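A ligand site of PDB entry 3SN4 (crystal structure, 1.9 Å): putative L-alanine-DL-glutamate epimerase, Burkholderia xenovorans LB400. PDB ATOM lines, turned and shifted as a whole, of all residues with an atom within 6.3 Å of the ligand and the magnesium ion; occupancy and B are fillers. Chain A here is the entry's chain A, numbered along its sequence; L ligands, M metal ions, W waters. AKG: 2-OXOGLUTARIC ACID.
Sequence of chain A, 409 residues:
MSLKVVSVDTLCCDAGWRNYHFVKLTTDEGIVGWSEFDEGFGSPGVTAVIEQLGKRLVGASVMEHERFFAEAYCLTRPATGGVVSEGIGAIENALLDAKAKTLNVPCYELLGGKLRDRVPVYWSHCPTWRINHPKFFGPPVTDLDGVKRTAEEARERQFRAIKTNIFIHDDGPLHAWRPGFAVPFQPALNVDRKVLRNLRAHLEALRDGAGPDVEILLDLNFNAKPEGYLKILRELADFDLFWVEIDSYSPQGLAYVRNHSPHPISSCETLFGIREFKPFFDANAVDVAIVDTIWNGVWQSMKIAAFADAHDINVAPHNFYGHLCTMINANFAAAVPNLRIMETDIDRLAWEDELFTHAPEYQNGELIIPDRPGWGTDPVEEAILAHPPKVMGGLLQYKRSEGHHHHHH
An oxygen (O1) of the ligand lies close to the side-chain carboxylate (OE2) of Glu 343, at 2.7 Å.
O5 of the ligand sits close to ND2 of Asn 221, at 2.7 Å.
The side-chain amino group (NZ) of Lys 163 lies close to an oxygen (O2) of the ligand (2.7 Å).
NE2 of His 318 lies within hydrogen-bond range of O1 of the ligand, at 3.2 Å.
A ring nitrogen (NE2) of His 125 lies within hydrogen-bond range of an oxygen (O3) of the ligand, at 3.2 Å.
NH2 of Arg 178 lies within salt-bridge range of O4 of the ligand (3.3 Å).
The side-chain carboxylate of Glu 245 is in salt-bridge range of the side-chain amino group of Lys 163 (2.8 Å).
N of Asn 221 sits at hydrogen-bond distance from OD1 of Asp 219, 2.8 Å away.
The side-chain amino group (NZ) of Lys 163 sits close to the side-chain carboxylate (OD2) of Asp 219.
The side-chain amide oxygen (OD1) of Asn 221 is in hydrogen-bond range of the side-chain amide nitrogen (ND2) of Asn 165.
The backbone carbonyl oxygen (O) of Asn 221 sits at hydrogen-bond distance from the backbone NH (N) of Asp 247 (2.9 Å).
The backbone carbonyl oxygen (O) of Lys 163 lies within hydrogen-bond range of the backbone NH (N) of His 125 (3.1 Å).
A ring nitrogen (ND1) of His 125 is in hydrogen-bond range of the side-chain hydroxyl (OG) of Ser 124 (3.3 Å).
The side-chain carboxylate of Asp 345 is in hydrogen-bond range of a ring nitrogen (ND1) of His 125 (2.7 Å).
CZ of Phe 41 touches C3 of the ligand, 3.9 Å away.
Asn 165 touches the ligand.
Phe 181 touches the ligand.
CE1 of Phe 320 touches C4 of the ligand, at 3.4 Å.
Of the 22 residues printed, 13 come within 4 Å of the ligand.
Residues that only touch the magnesium ion: Asn 221 (3.7 Å).
Four residues have an atom within 4 Å of the magnesium ion: Asp 219, Asn 221, Glu 245 and Glu 269.
The magnesium ion is bound by water W2, OE1 of Glu 245, OD2 of Asp 219, O5 of the ligand, OE2 of Glu 269 and O2 of the ligand.
The magnesium ion has six donor atoms within binding distance.
Water W3 lies within hydrogen-bond range of O3 of the ligand (2.9 Å), ND2 of Asn 165 (2.9 Å) and NE2 of His 125 (3.4 Å).
Water W1 lies within hydrogen-bond range of NZ of Lys 163, OE1 of Glu 343 and OH of Tyr 122.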
ATOM      1  N   PHE A  41      19.555  19.790  11.981  1.00  0.00           N
ATOM      2  CA  PHE A  41      20.753  19.770  12.830  1.00  0.00           C
ATOM      3  C   PHE A  41      21.059  21.164  13.346  1.00  0.00           C
ATOM      4  O   PHE A  41      22.037  21.819  12.951  1.00  0.00           O
ATOM      5  CB  PHE A  41      21.943  19.171  12.100  1.00  0.00           C
ATOM      6  CG  PHE A  41      23.093  18.776  13.011  1.00  0.00           C
ATOM      7  CD1 PHE A  41      22.857  18.050  14.184  1.00  0.00           C
ATOM      8  CD2 PHE A  41      24.402  19.099  12.699  1.00  0.00           C
ATOM      9  CE1 PHE A  41      23.900  17.671  15.011  1.00  0.00           C
ATOM     10  CE2 PHE A  41      25.463  18.711  13.536  1.00  0.00           C
ATOM     11  CZ  PHE A  41      25.199  18.016  14.697  1.00  0.00           C
ATOM     12  N   TYR A 122      33.380   4.463   6.995  1.00  0.00           N
ATOM     13  CA  TYR A 122      32.838   3.811   8.173  1.00  0.00           C
ATOM     14  C   TYR A 122      31.314   3.914   8.194  1.00  0.00           C
ATOM     15  O   TYR A 122      30.737   4.889   7.722  1.00  0.00           O
ATOM     16  CB  TYR A 122      33.420   4.372   9.464  1.00  0.00           C
ATOM     17  CG  TYR A 122      33.100   5.791   9.789  1.00  0.00           C
ATOM     18  CD1 TYR A 122      32.063   6.114  10.665  1.00  0.00           C
ATOM     19  CD2 TYR A 122      33.886   6.831   9.285  1.00  0.00           C
ATOM     20  CE1 TYR A 122      31.799   7.452  11.018  1.00  0.00           C
ATOM     21  CE2 TYR A 122      33.616   8.166   9.626  1.00  0.00           C
ATOM     22  CZ  TYR A 122      32.593   8.455  10.497  1.00  0.00           C
ATOM     23  OH  TYR A 122      32.357   9.746  10.809  1.00  0.00           O
ATOM     24  N   SER A 124      28.346   4.755   9.950  1.00  0.00           N
ATOM     25  CA  SER A 124      28.121   5.697  11.023  1.00  0.00           C
ATOM     26  C   SER A 124      26.780   5.460  11.645  1.00  0.00           C
ATOM     27  O   SER A 124      25.930   4.773  11.070  1.00  0.00           O
ATOM     28  CB  SER A 124      28.197   7.123  10.488  1.00  0.00           C
ATOM     29  OG  SER A 124      28.213   7.996  11.583  1.00  0.00           O
ATOM     30  N   HIS A 125      26.614   6.020  12.862  1.00  0.00           N
ATOM     31  CA  HIS A 125      25.393   5.845  13.661  1.00  0.00           C
ATOM     32  C   HIS A 125      25.003   4.369  13.752  1.00  0.00           C
ATOM     33  O   HIS A 125      23.855   3.995  13.491  1.00  0.00           O
ATOM     34  CB  HIS A 125      24.247   6.669  13.060  1.00  0.00           C
ATOM     35  CG  HIS A 125      24.545   8.129  13.061  1.00  0.00           C
ATOM     36  ND1 HIS A 125      25.025   8.788  11.957  1.00  0.00           N
ATOM     37  CD2 HIS A 125      24.501   9.032  14.064  1.00  0.00           C
ATOM     38  CE1 HIS A 125      25.233  10.057  12.270  1.00  0.00           C
ATOM     39  NE2 HIS A 125      24.922  10.230  13.546  1.00  0.00           N
ATOM     40  N   THR A 128      23.412   3.472  16.529  1.00  0.00           N
ATOM     41  CA  THR A 128      22.663   4.657  16.914  1.00  0.00           C
ATOM     42  C   THR A 128      21.297   4.827  16.228  1.00  0.00           C
ATOM     43  O   THR A 128      20.301   5.096  16.901  1.00  0.00           O
ATOM     44  CB  THR A 128      23.518   5.926  16.702  1.00  0.00           C
ATOM     45  OG1 THR A 128      24.832   5.679  17.256  1.00  0.00           O
ATOM     46  CG2 THR A 128      22.843   7.152  17.353  1.00  0.00           C
ATOM     47  N   TRP A 129      21.257   4.677  14.910  1.00  0.00           N
ATOM     48  CA  TRP A 129      20.001   4.850  14.167  1.00  0.00           C
ATOM     49  C   TRP A 129      18.969   3.768  14.559  1.00  0.00           C
ATOM     50  O   TRP A 129      17.757   4.057  14.704  1.00  0.00           O
ATOM     51  CB  TRP A 129      20.285   4.788  12.659  1.00  0.00           C
ATOM     52  CG  TRP A 129      20.638   6.128  11.928  1.00  0.00           C
ATOM     53  CD1 TRP A 129      20.795   6.268  10.560  1.00  0.00           C
ATOM     54  CD2 TRP A 129      20.842   7.440  12.486  1.00  0.00           C
ATOM     55  NE1 TRP A 129      21.089   7.569  10.238  1.00  0.00           N
ATOM     56  CE2 TRP A 129      21.138   8.309  11.393  1.00  0.00           C
ATOM     57  CE3 TRP A 129      20.829   7.966  13.778  1.00  0.00           C
ATOM     58  CZ2 TRP A 129      21.412   9.667  11.567  1.00  0.00           C
ATOM     59  CZ3 TRP A 129      21.101   9.313  13.955  1.00  0.00           C
ATOM     60  CH2 TRP A 129      21.395  10.157  12.846  1.00  0.00           C
ATOM     61  N   LYS A 163      30.800   3.531  13.769  1.00  0.00           N
ATOM     62  CA  LYS A 163      30.777   4.619  14.763  1.00  0.00           C
ATOM     63  C   LYS A 163      29.503   4.600  15.578  1.00  0.00           C
ATOM     64  O   LYS A 163      28.403   4.593  15.018  1.00  0.00           O
ATOM     65  CB  LYS A 163      30.936   6.000  14.108  1.00  0.00           C
ATOM     66  CG  LYS A 163      31.257   7.094  15.130  1.00  0.00           C
ATOM     67  CD  LYS A 163      31.727   8.414  14.512  1.00  0.00           C
ATOM     68  CE  LYS A 163      30.544   9.264  14.023  1.00  0.00           C
ATOM     69  NZ  LYS A 163      30.980  10.408  13.155  1.00  0.00           N
ATOM     70  N   ASN A 165      27.554   6.141  19.476  1.00  0.00           N
ATOM     71  CA  ASN A 165      27.404   7.324  20.327  1.00  0.00           C
ATOM     72  C   ASN A 165      27.249   6.886  21.787  1.00  0.00           C
ATOM     73  O   ASN A 165      27.825   5.881  22.155  1.00  0.00           O
ATOM     74  CB  ASN A 165      26.231   8.184  19.838  1.00  0.00           C
ATOM     75  CG  ASN A 165      26.387   8.577  18.406  1.00  0.00           C
ATOM     76  OD1 ASN A 165      26.110   7.775  17.495  1.00  0.00           O
ATOM     77  ND2 ASN A 165      26.801   9.818  18.166  1.00  0.00           N
ATOM     78  N   ARG A 178      22.112  12.486  25.306  1.00  0.00           N
ATOM     79  CA  ARG A 178      22.421  13.611  24.404  1.00  0.00           C
ATOM     80  C   ARG A 178      22.172  14.976  25.061  1.00  0.00           C
ATOM     81  O   ARG A 178      21.500  15.834  24.487  1.00  0.00           O
ATOM     82  CB  ARG A 178      21.573  13.501  23.132  1.00  0.00           C
ATOM     83  CG  ARG A 178      22.005  12.358  22.226  1.00  0.00           C
ATOM     84  CD  ARG A 178      20.898  11.878  21.313  1.00  0.00           C
ATOM     85  NE  ARG A 178      20.336  12.925  20.459  1.00  0.00           N
ATOM     86  CZ  ARG A 178      20.943  13.458  19.395  1.00  0.00           C
ATOM     87  NH1 ARG A 178      20.313  14.398  18.685  1.00  0.00           N
ATOM     88  NH2 ARG A 178      22.185  13.068  19.025  1.00  0.00           N
ATOM     89  N   PHE A 181      22.419  18.379  23.411  1.00  0.00           N
ATOM     90  CA  PHE A 181      21.276  18.758  22.588  1.00  0.00           C
ATOM     91  C   PHE A 181      19.954  18.751  23.390  1.00  0.00           C
ATOM     92  O   PHE A 181      18.840  18.655  22.843  1.00  0.00           O
ATOM     93  CB  PHE A 181      21.205  17.812  21.370  1.00  0.00           C
ATOM     94  CG  PHE A 181      22.436  17.810  20.476  1.00  0.00           C
ATOM     95  CD1 PHE A 181      23.165  18.977  20.235  1.00  0.00           C
ATOM     96  CD2 PHE A 181      22.813  16.642  19.783  1.00  0.00           C
ATOM     97  CE1 PHE A 181      24.270  18.991  19.385  1.00  0.00           C
ATOM     98  CE2 PHE A 181      23.911  16.643  18.923  1.00  0.00           C
ATOM     99  CZ  PHE A 181      24.658  17.819  18.720  1.00  0.00           C
ATOM    100  N   ASP A 219      31.662   8.762  19.003  1.00  0.00           N
ATOM    101  CA  ASP A 219      31.300  10.173  18.904  1.00  0.00           C
ATOM    102  C   ASP A 219      30.612  10.595  20.188  1.00  0.00           C
ATOM    103  O   ASP A 219      29.589  10.017  20.583  1.00  0.00           O
ATOM    104  CB  ASP A 219      30.405  10.413  17.698  1.00  0.00           C
ATOM    105  CG  ASP A 219      30.278  11.893  17.310  1.00  0.00           C
ATOM    106  OD1 ASP A 219      30.603  12.811  18.098  1.00  0.00           O
ATOM    107  OD2 ASP A 219      29.809  12.121  16.172  1.00  0.00           O
ATOM    108  N   ASN A 221      30.035  14.019  20.573  1.00  0.00           N
ATOM    109  CA  ASN A 221      29.344  15.243  20.128  1.00  0.00           C
ATOM    110  C   ASN A 221      29.638  16.390  21.109  1.00  0.00           C
ATOM    111  O   ASN A 221      30.796  16.558  21.491  1.00  0.00           O
ATOM    112  CB  ASN A 221      27.836  15.000  19.944  1.00  0.00           C
ATOM    113  CG  ASN A 221      27.528  13.958  18.886  1.00  0.00           C
ATOM    114  OD1 ASN A 221      27.282  12.801  19.213  1.00  0.00           O
ATOM    115  ND2 ASN A 221      27.525  14.378  17.628  1.00  0.00           N
ATOM    116  N   GLU A 245      35.446  11.394  18.948  1.00  0.00           N
ATOM    117  CA  GLU A 245      34.986  12.600  18.310  1.00  0.00           C
ATOM    118  C   GLU A 245      34.350  13.471  19.360  1.00  0.00           C
ATOM    119  O   GLU A 245      33.489  13.028  20.117  1.00  0.00           O
ATOM    120  CB  GLU A 245      33.986  12.219  17.238  1.00  0.00           C
ATOM    121  CG  GLU A 245      33.610  13.282  16.218  1.00  0.00           C
ATOM    122  CD  GLU A 245      32.835  12.667  15.035  1.00  0.00           C
ATOM    123  OE1 GLU A 245      32.008  13.360  14.452  1.00  0.00           O
ATOM    124  OE2 GLU A 245      33.049  11.470  14.715  1.00  0.00           O
ATOM    125  N   ASP A 247      32.999  17.559  19.854  1.00  0.00           N
ATOM    126  CA  ASP A 247      32.764  18.913  19.396  1.00  0.00           C
ATOM    127  C   ASP A 247      32.870  19.924  20.527  1.00  0.00           C
ATOM    128  O   ASP A 247      32.340  19.696  21.622  1.00  0.00           O
ATOM    129  CB  ASP A 247      31.411  19.026  18.734  1.00  0.00           C
ATOM    130  CG  ASP A 247      31.283  18.135  17.542  1.00  0.00           C
ATOM    131  OD1 ASP A 247      32.126  18.224  16.614  1.00  0.00           O
ATOM    132  OD2 ASP A 247      30.332  17.343  17.563  1.00  0.00           O
ATOM    133  N   GLU A 269      33.317  19.347  12.956  1.00  0.00           N
ATOM    134  CA  GLU A 269      32.239  19.141  11.984  1.00  0.00           C
ATOM    135  C   GLU A 269      31.285  20.311  11.868  1.00  0.00           C
ATOM    136  O   GLU A 269      30.541  20.433  10.879  1.00  0.00           O
ATOM    137  CB  GLU A 269      31.441  17.854  12.294  1.00  0.00           C
ATOM    138  CG  GLU A 269      30.421  17.971  13.431  1.00  0.00           C
ATOM    139  CD  GLU A 269      29.792  16.651  13.857  1.00  0.00           C
ATOM    140  OE1 GLU A 269      28.664  16.689  14.418  1.00  0.00           O
ATOM    141  OE2 GLU A 269      30.395  15.561  13.640  1.00  0.00           O
ATOM    142  N   ILE A 290      37.194  16.990  10.916  1.00  0.00           N
ATOM    143  CA  ILE A 290      35.956  16.638  10.212  1.00  0.00           C
ATOM    144  C   ILE A 290      35.486  17.901   9.515  1.00  0.00           C
ATOM    145  O   ILE A 290      35.402  18.955  10.132  1.00  0.00           O
ATOM    146  CB  ILE A 290      34.916  16.065  11.177  1.00  0.00           C
ATOM    147  CG1 ILE A 290      35.455  14.722  11.735  1.00  0.00           C
ATOM    148  CG2 ILE A 290      33.560  15.827  10.463  1.00  0.00           C
ATOM    149  CD1 ILE A 290      34.722  14.181  12.977  1.00  0.00           C
ATOM    150  N   HIS A 318      31.904  15.154   6.842  1.00  0.00           N
ATOM    151  CA  HIS A 318      30.715  14.936   7.646  1.00  0.00           C
ATOM    152  C   HIS A 318      29.578  14.582   6.723  1.00  0.00           C
ATOM    153  O   HIS A 318      29.171  15.402   5.898  1.00  0.00           O
ATOM    154  CB  HIS A 318      30.395  16.235   8.376  1.00  0.00           C
ATOM    155  CG  HIS A 318      29.413  16.068   9.488  1.00  0.00           C
ATOM    156  ND1 HIS A 318      28.658  17.120   9.949  1.00  0.00           N
ATOM    157  CD2 HIS A 318      29.048  14.978  10.208  1.00  0.00           C
ATOM    158  CE1 HIS A 318      27.893  16.697  10.945  1.00  0.00           C
ATOM    159  NE2 HIS A 318      28.099  15.392  11.101  1.00  0.00           N
ATOM    160  N   ASN A 319      29.051  13.377   6.869  1.00  0.00           N
ATOM    161  CA  ASN A 319      28.078  12.854   5.924  1.00  0.00           C
ATOM    162  C   ASN A 319      27.082  11.971   6.639  1.00  0.00           C
ATOM    163  O   ASN A 319      27.365  10.781   6.891  1.00  0.00           O
ATOM    164  CB  ASN A 319      28.814  12.043   4.862  1.00  0.00           C
ATOM    165  CG  ASN A 319      27.916  11.579   3.758  1.00  0.00           C
ATOM    166  OD1 ASN A 319      27.191  12.383   3.157  1.00  0.00           O
ATOM    167  ND2 ASN A 319      27.948  10.272   3.467  1.00  0.00           N
ATOM    168  N   PHE A 320      25.928  12.547   6.994  1.00  0.00           N
ATOM    169  CA  PHE A 320      24.887  11.787   7.682  1.00  0.00           C
ATOM    170  C   PHE A 320      23.482  12.169   7.236  1.00  0.00           C
ATOM    171  O   PHE A 320      22.515  12.159   8.040  1.00  0.00           O
ATOM    172  CB  PHE A 320      25.044  11.876   9.217  1.00  0.00           C
ATOM    173  CG  PHE A 320      24.574  13.178   9.838  1.00  0.00           C
ATOM    174  CD1 PHE A 320      23.493  13.200  10.708  1.00  0.00           C
ATOM    175  CD2 PHE A 320      25.234  14.378   9.579  1.00  0.00           C
ATOM    176  CE1 PHE A 320      23.054  14.402  11.284  1.00  0.00           C
ATOM    177  CE2 PHE A 320      24.791  15.573  10.167  1.00  0.00           C
ATOM    178  CZ  PHE A 320      23.707  15.579  11.019  1.00  0.00           C
ATOM    179  N   GLU A 343      32.644   9.146   6.111  1.00  0.00           N
ATOM    180  CA  GLU A 343      31.475   8.764   6.901  1.00  0.00           C
ATOM    181  C   GLU A 343      30.342   8.407   5.969  1.00  0.00           C
ATOM    182  O   GLU A 343      30.106   9.066   4.975  1.00  0.00           O
ATOM    183  CB  GLU A 343      31.017   9.929   7.766  1.00  0.00           C
ATOM    184  CG  GLU A 343      29.802   9.618   8.637  1.00  0.00           C
ATOM    185  CD  GLU A 343      29.439  10.747   9.588  1.00  0.00           C
ATOM    186  OE1 GLU A 343      29.811  11.920   9.321  1.00  0.00           O
ATOM    187  OE2 GLU A 343      28.797  10.438  10.619  1.00  0.00           O
ATOM    188  N   ASP A 345      26.107   6.691   6.409  1.00  0.00           N
ATOM    189  CA  ASP A 345      25.039   5.967   7.107  1.00  0.00           C
ATOM    190  C   ASP A 345      24.573   4.806   6.229  1.00  0.00           C
ATOM    191  O   ASP A 345      24.003   4.990   5.155  1.00  0.00           O
ATOM    192  CB  ASP A 345      23.878   6.879   7.458  1.00  0.00           C
ATOM    193  CG  ASP A 345      24.205   7.896   8.577  1.00  0.00           C
ATOM    194  OD1 ASP A 345      25.007   7.605   9.512  1.00  0.00           O
ATOM    195  OD2 ASP A 345      23.595   8.997   8.549  1.00  0.00           O
ATOM    196  N   LEU A 395      17.194  17.938  15.797  1.00  0.00           N
ATOM    197  CA  LEU A 395      17.374  18.459  17.172  1.00  0.00           C
ATOM    198  C   LEU A 395      16.158  19.210  17.668  1.00  0.00           C
ATOM    199  O   LEU A 395      15.928  19.294  18.884  1.00  0.00           O
ATOM    200  CB  LEU A 395      18.592  19.403  17.257  1.00  0.00           C
ATOM    201  CG  LEU A 395      19.911  18.841  16.761  1.00  0.00           C
ATOM    202  CD1 LEU A 395      21.043  19.806  17.133  1.00  0.00           C
ATOM    203  CD2 LEU A 395      20.149  17.395  17.298  1.00  0.00           C
HETATM  204  C1  AKG L   1      28.148  12.837  12.983  1.00  0.00           C
HETATM  205  O1  AKG L   1      27.575  12.386  11.954  1.00  0.00           O
HETATM  206  O2  AKG L   1      29.379  12.575  13.212  1.00  0.00           O
HETATM  207  C2  AKG L   1      27.413  13.719  13.931  1.00  0.00           C
HETATM  208  O5  AKG L   1      27.913  14.026  15.013  1.00  0.00           O
HETATM  209  C3  AKG L   1      26.080  14.352  13.612  1.00  0.00           C
HETATM  210  C4  AKG L   1      24.789  13.674  14.111  1.00  0.00           C
HETATM  211  C5  AKG L   1      24.600  13.293  15.571  1.00  0.00           C
HETATM  212  O3  AKG L   1      25.204  12.275  15.978  1.00  0.00           O
HETATM  213  O4  AKG L   1      23.802  13.965  16.292  1.00  0.00           O
HETATM  214 MG    MG M   1      30.032  13.847  14.971  1.00  0.00          MG
HETATM  215  O   HOH W   1      31.863  13.005  11.581  1.00  0.00           O
HETATM  216  O   HOH W   2      30.476  15.013  16.589  1.00  0.00           O
HETATM  217  O   HOH W   3      27.602  10.759  15.521  1.00  0.00           O
